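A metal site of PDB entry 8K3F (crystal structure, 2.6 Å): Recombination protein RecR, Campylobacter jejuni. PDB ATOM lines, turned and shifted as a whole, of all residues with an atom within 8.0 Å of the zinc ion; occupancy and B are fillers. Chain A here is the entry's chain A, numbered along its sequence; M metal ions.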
ATOM      1  N   PRO A  63      -9.630  17.514  10.886  1.00  0.00           N
ATOM      2  CA  PRO A  63      -9.084  18.813  11.293  1.00  0.00           C
ATOM      3  C   PRO A  63      -8.449  18.715  12.671  1.00  0.00           C
ATOM      4  O   PRO A  63      -8.976  18.043  13.564  1.00  0.00           O
ATOM      5  CB  PRO A  63     -10.315  19.737  11.304  1.00  0.00           C
ATOM      6  CG  PRO A  63     -11.327  19.041  10.429  1.00  0.00           C
ATOM      7  CD  PRO A  63     -11.091  17.580  10.697  1.00  0.00           C
ATOM      8  N   CYS A  64      -7.322  19.385  12.831  1.00  0.00           N
ATOM      9  CA  CYS A  64      -6.699  19.465  14.143  1.00  0.00           C
ATOM     10  C   CYS A  64      -7.655  20.111  15.130  1.00  0.00           C
ATOM     11  O   CYS A  64      -8.236  21.165  14.845  1.00  0.00           O
ATOM     12  CB  CYS A  64      -5.391  20.250  14.057  1.00  0.00           C
ATOM     13  SG  CYS A  64      -4.632  20.580  15.645  1.00  0.00           S
ATOM     14  N   GLU A  65      -7.800  19.491  16.303  1.00  0.00           N
ATOM     15  CA  GLU A  65      -8.788  19.963  17.272  1.00  0.00           C
ATOM     16  C   GLU A  65      -8.474  21.376  17.755  1.00  0.00           C
ATOM     17  O   GLU A  65      -9.386  22.110  18.153  1.00  0.00           O
ATOM     18  CB  GLU A  65      -8.858  19.008  18.460  1.00  0.00           C
ATOM     19  N   GLN A  66      -7.203  21.782  17.732  1.00  0.00           N
ATOM     20  CA  GLN A  66      -6.802  23.110  18.183  1.00  0.00           C
ATOM     21  C   GLN A  66      -6.902  24.152  17.073  1.00  0.00           C
ATOM     22  O   GLN A  66      -7.606  25.159  17.205  1.00  0.00           O
ATOM     23  CB  GLN A  66      -5.389  23.042  18.757  1.00  0.00           C
ATOM     24  CG  GLN A  66      -4.809  24.393  19.125  1.00  0.00           C
ATOM     25  CD  GLN A  66      -3.953  24.341  20.369  1.00  0.00           C
ATOM     26  OE1 GLN A  66      -4.448  24.080  21.473  1.00  0.00           O
ATOM     27  NE2 GLN A  66      -2.655  24.589  20.202  1.00  0.00           N
ATOM     28  N   CYS A  67      -6.193  23.925  15.963  1.00  0.00           N
ATOM     29  CA  CYS A  67      -5.972  24.957  14.948  1.00  0.00           C
ATOM     30  C   CYS A  67      -6.753  24.756  13.661  1.00  0.00           C
ATOM     31  O   CYS A  67      -6.943  25.721  12.920  1.00  0.00           O
ATOM     32  CB  CYS A  67      -4.478  25.025  14.608  1.00  0.00           C
ATOM     33  SG  CYS A  67      -3.896  23.617  13.667  1.00  0.00           S
ATOM     34  N   GLY A  68      -7.152  23.528  13.342  1.00  0.00           N
ATOM     35  CA  GLY A  68      -7.918  23.277  12.140  1.00  0.00           C
ATOM     36  C   GLY A  68      -7.102  22.747  10.992  1.00  0.00           C
ATOM     37  O   GLY A  68      -7.655  22.530   9.907  1.00  0.00           O
ATOM     38  N   ALA A  69      -5.811  22.506  11.187  1.00  0.00           N
ATOM     39  CA  ALA A  69      -4.953  22.063  10.105  1.00  0.00           C
ATOM     40  C   ALA A  69      -5.261  20.618   9.723  1.00  0.00           C
ATOM     41  O   ALA A  69      -6.038  19.928  10.389  1.00  0.00           O
ATOM     42  CB  ALA A  69      -3.479  22.196  10.502  1.00  0.00           C
ATOM     43  N   LEU A  70      -4.647  20.166   8.640  1.00  0.00           N
ATOM     44  CA  LEU A  70      -4.726  18.756   8.295  1.00  0.00           C
ATOM     45  C   LEU A  70      -4.051  17.941   9.399  1.00  0.00           C
ATOM     46  O   LEU A  70      -2.923  18.232   9.793  1.00  0.00           O
ATOM     47  CB  LEU A  70      -4.033  18.508   6.964  1.00  0.00           C
ATOM     48  CG  LEU A  70      -4.918  18.725   5.729  1.00  0.00           C
ATOM     49  CD1 LEU A  70      -4.184  18.323   4.460  1.00  0.00           C
ATOM     50  CD2 LEU A  70      -6.194  17.954   5.893  1.00  0.00           C
ATOM     51  N   SER A  71      -4.743  16.919   9.888  1.00  0.00           N
ATOM     52  CA  SER A  71      -4.184  16.129  10.967  1.00  0.00           C
ATOM     53  C   SER A  71      -4.621  14.676  10.842  1.00  0.00           C
ATOM     54  O   SER A  71      -5.651  14.359  10.244  1.00  0.00           O
ATOM     55  CB  SER A  71      -4.610  16.674  12.332  1.00  0.00           C
ATOM     56  OG  SER A  71      -3.817  16.131  13.361  1.00  0.00           O
ATOM     57  N   ASN A  73      -4.073  12.927  13.953  1.00  0.00           N
ATOM     58  CA  ASN A  73      -4.292  12.738  15.377  1.00  0.00           C
ATOM     59  C   ASN A  73      -5.228  13.834  15.884  1.00  0.00           C
ATOM     60  O   ASN A  73      -5.727  14.662  15.111  1.00  0.00           O
ATOM     61  CB  ASN A  73      -2.952  12.761  16.122  1.00  0.00           C
ATOM     62  CG  ASN A  73      -2.017  11.663  15.661  1.00  0.00           C
ATOM     63  OD1 ASN A  73      -2.268  10.470  15.878  1.00  0.00           O
ATOM     64  ND2 ASN A  73      -0.932  12.056  15.010  1.00  0.00           N
ATOM     65  N   GLU A  74      -5.435  13.875  17.205  1.00  0.00           N
ATOM     66  CA  GLU A  74      -6.283  14.919  17.754  1.00  0.00           C
ATOM     67  C   GLU A  74      -5.610  16.279  17.648  1.00  0.00           C
ATOM     68  O   GLU A  74      -6.256  17.286  17.340  1.00  0.00           O
ATOM     69  CB  GLU A  74      -6.626  14.594  19.215  1.00  0.00           C
ATOM     70  CG  GLU A  74      -7.305  15.729  19.995  1.00  0.00           C
ATOM     71  CD  GLU A  74      -8.773  15.911  19.645  1.00  0.00           C
ATOM     72  OE1 GLU A  74      -9.241  15.341  18.636  1.00  0.00           O
ATOM     73  OE2 GLU A  74      -9.464  16.631  20.400  1.00  0.00           O
ATOM     74  N   LEU A  75      -4.297  16.324  17.868  1.00  0.00           N
ATOM     75  CA  LEU A  75      -3.481  17.498  17.634  1.00  0.00           C
ATOM     76  C   LEU A  75      -2.562  17.244  16.446  1.00  0.00           C
ATOM     77  O   LEU A  75      -2.022  16.140  16.295  1.00  0.00           O
ATOM     78  CB  LEU A  75      -2.660  17.855  18.868  1.00  0.00           C
ATOM     79  CG  LEU A  75      -3.420  18.344  20.113  1.00  0.00           C
ATOM     80  CD1 LEU A  75      -2.525  19.226  20.958  1.00  0.00           C
ATOM     81  CD2 LEU A  75      -4.686  19.092  19.722  1.00  0.00           C
ATOM     82  N   CYS A  76      -2.371  18.266  15.618  1.00  0.00           N
ATOM     83  CA  CYS A  76      -1.463  18.156  14.490  1.00  0.00           C
ATOM     84  C   CYS A  76      -0.021  18.159  14.995  1.00  0.00           C
ATOM     85  O   CYS A  76       0.258  18.326  16.191  1.00  0.00           O
ATOM     86  CB  CYS A  76      -1.686  19.295  13.500  1.00  0.00           C
ATOM     87  SG  CYS A  76      -1.218  20.942  14.120  1.00  0.00           S
ATOM     88  N   GLU A  77       0.910  17.949  14.062  1.00  0.00           N
ATOM     89  CA  GLU A  77       2.323  17.909  14.447  1.00  0.00           C
ATOM     90  C   GLU A  77       2.853  19.281  14.824  1.00  0.00           C
ATOM     91  O   GLU A  77       3.803  19.387  15.606  1.00  0.00           O
ATOM     92  CB  GLU A  77       3.174  17.315  13.321  1.00  0.00           C
ATOM     93  CG  GLU A  77       3.081  15.790  13.195  1.00  0.00           C
ATOM     94  CD  GLU A  77       3.423  15.079  14.495  1.00  0.00           C
ATOM     95  OE1 GLU A  77       2.494  14.689  15.229  1.00  0.00           O
ATOM     96  OE2 GLU A  77       4.637  14.901  14.775  1.00  0.00           O
ATOM     97  N   ILE A  78       2.261  20.348  14.291  1.00  0.00           N
ATOM     98  CA  ILE A  78       2.717  21.686  14.652  1.00  0.00           C
ATOM     99  C   ILE A  78       2.271  22.031  16.065  1.00  0.00           C
ATOM    100  O   ILE A  78       3.074  22.494  16.890  1.00  0.00           O
ATOM    101  CB  ILE A  78       2.218  22.728  13.640  1.00  0.00           C
ATOM    102  CG1 ILE A  78       2.885  22.496  12.273  1.00  0.00           C
ATOM    103  CG2 ILE A  78       2.504  24.131  14.132  1.00  0.00           C
ATOM    104  CD1 ILE A  78       2.162  23.188  11.121  1.00  0.00           C
ATOM    105  N   CYS A  79       1.000  21.771  16.399  1.00  0.00           N
ATOM    106  CA  CYS A  79       0.509  22.067  17.730  1.00  0.00           C
ATOM    107  C   CYS A  79       1.096  21.161  18.789  1.00  0.00           C
ATOM    108  O   CYS A  79       0.999  21.472  19.983  1.00  0.00           O
ATOM    109  CB  CYS A  79      -1.014  21.965  17.770  1.00  0.00           C
ATOM    110  SG  CYS A  79      -1.879  23.214  16.825  1.00  0.00           S
ATOM    111  N   SER A  80       1.706  20.042  18.390  1.00  0.00           N
ATOM    112  CA  SER A  80       2.331  19.112  19.309  1.00  0.00           C
ATOM    113  C   SER A  80       3.834  19.348  19.457  1.00  0.00           C
ATOM    114  O   SER A  80       4.473  18.686  20.289  1.00  0.00           O
ATOM    115  CB  SER A  80       2.102  17.672  18.847  1.00  0.00           C
ATOM    116  OG  SER A  80       0.724  17.353  18.838  1.00  0.00           O
ATOM    117  N   ILE A  98      -1.477  26.469   5.390  1.00  0.00           N
ATOM    118  CA  ILE A  98      -0.437  26.057   6.322  1.00  0.00           C
ATOM    119  C   ILE A  98       0.625  25.231   5.608  1.00  0.00           C
ATOM    120  O   ILE A  98       1.825  25.438   5.818  1.00  0.00           O
ATOM    121  CB  ILE A  98      -1.048  25.295   7.501  1.00  0.00           C
ATOM    122  CG1 ILE A  98      -2.068  26.174   8.229  1.00  0.00           C
ATOM    123  CG2 ILE A  98       0.040  24.885   8.479  1.00  0.00           C
ATOM    124  CD1 ILE A  98      -2.864  25.424   9.267  1.00  0.00           C
ATOM    125  N   LEU A 110       2.577  29.213  15.624  1.00  0.00           N
ATOM    126  CA  LEU A 110       1.398  28.375  15.514  1.00  0.00           C
ATOM    127  C   LEU A 110       0.444  28.984  14.491  1.00  0.00           C
ATOM    128  O   LEU A 110       0.531  30.175  14.148  1.00  0.00           O
ATOM    129  CB  LEU A 110       0.711  28.205  16.863  1.00  0.00           C
ATOM    130  CG  LEU A 110       1.603  27.580  17.935  1.00  0.00           C
ATOM    131  CD1 LEU A 110       1.051  27.864  19.326  1.00  0.00           C
ATOM    132  CD2 LEU A 110       1.758  26.077  17.715  1.00  0.00           C
ATOM    133  N   TYR A 111      -0.473  28.169  14.007  1.00  0.00           N
ATOM    134  CA  TYR A 111      -1.441  28.593  13.015  1.00  0.00           C
ATOM    135  C   TYR A 111      -2.847  28.464  13.578  1.00  0.00           C
ATOM    136  O   TYR A 111      -3.095  27.684  14.496  1.00  0.00           O
ATOM    137  CB  TYR A 111      -1.345  27.772  11.726  1.00  0.00           C
ATOM    138  CG  TYR A 111      -0.016  27.815  11.004  1.00  0.00           C
ATOM    139  CD1 TYR A 111       0.967  26.881  11.269  1.00  0.00           C
ATOM    140  CD2 TYR A 111       0.233  28.782  10.036  1.00  0.00           C
ATOM    141  CE1 TYR A 111       2.172  26.913  10.593  1.00  0.00           C
ATOM    142  CE2 TYR A 111       1.437  28.823   9.356  1.00  0.00           C
ATOM    143  CZ  TYR A 111       2.402  27.884   9.638  1.00  0.00           C
ATOM    144  OH  TYR A 111       3.600  27.898   8.972  1.00  0.00           O
ATOM    145  N   PHE A 112      -3.769  29.212  12.998  1.00  0.00           N
ATOM    146  CA  PHE A 112      -5.177  29.060  13.306  1.00  0.00           C
ATOM    147  C   PHE A 112      -5.941  29.182  12.005  1.00  0.00           C
ATOM    148  O   PHE A 112      -5.746  30.155  11.264  1.00  0.00           O
ATOM    149  CB  PHE A 112      -5.646  30.121  14.305  1.00  0.00           C
ATOM    150  CG  PHE A 112      -7.045  29.902  14.786  1.00  0.00           C
ATOM    151  CD1 PHE A 112      -7.310  28.966  15.776  1.00  0.00           C
ATOM    152  CD2 PHE A 112      -8.096  30.605  14.225  1.00  0.00           C
ATOM    153  CE1 PHE A 112      -8.605  28.758  16.212  1.00  0.00           C
ATOM    154  CE2 PHE A 112      -9.390  30.397  14.661  1.00  0.00           C
ATOM    155  CZ  PHE A 112      -9.644  29.464  15.659  1.00  0.00           C
ATOM    156  N   VAL A 113      -6.776  28.187  11.698  1.00  0.00           N
ATOM    157  CA  VAL A 113      -7.587  28.233  10.482  1.00  0.00           C
ATOM    158  C   VAL A 113      -8.882  28.957  10.826  1.00  0.00           C
ATOM    159  O   VAL A 113      -9.733  28.425  11.544  1.00  0.00           O
ATOM    160  CB  VAL A 113      -7.853  26.833   9.919  1.00  0.00           C
ATOM    161  CG1 VAL A 113      -8.691  26.935   8.661  1.00  0.00           C
ATOM    162  CG2 VAL A 113      -6.555  26.127   9.590  1.00  0.00           C
HETATM  163 ZN    ZN M   1      -2.933  22.048  15.070  1.00  0.00          ZN
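The backbone NH of Ala 69 lies close to the side-chain sulfur of Cys 67. The side-chain sulfur (SG) of Cys 76 sits close to the backbone NH (N) of Ile 78, 3.5 Å away. SG of Cys 79 lies close to NE2 of Gln 66 (3.7 Å). N of Cys 64 is in hydrogen-bond range of O of Ala 69. The backbone carbonyl oxygen (O) of Cys 67 sits at hydrogen-bond distance from the backbone NH (N) of Val 113 (2.8 Å). The side-chain sulfur of Cys 64 sits close to the backbone NH of Gln 66 (3.5 Å). OG of Ser 80 sits at hydrogen-bond distance from O of Cys 76 (2.9 Å). The backbone NH (N) of Cys 76 lies close to the side-chain hydroxyl (OG) of Ser 71 (3.4 Å).
The zinc ion is bound by the side-chain sulfur of Cys 76 (2.3 Å), the side-chain sulfur of Cys 67 (2.3 Å), the side-chain sulfur of Cys 64 (2.3 Å) and the side-chain sulfur of Cys 79 (2.4 Å). The zinc ion has four donor atoms within binding distance.
Within 4 Å of the zinc ion: Cys 64, Cys 67, Cys 76 and Cys 79. The nearest printed residue that does not touch the zinc ion is Gln 66 (4.5 Å).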
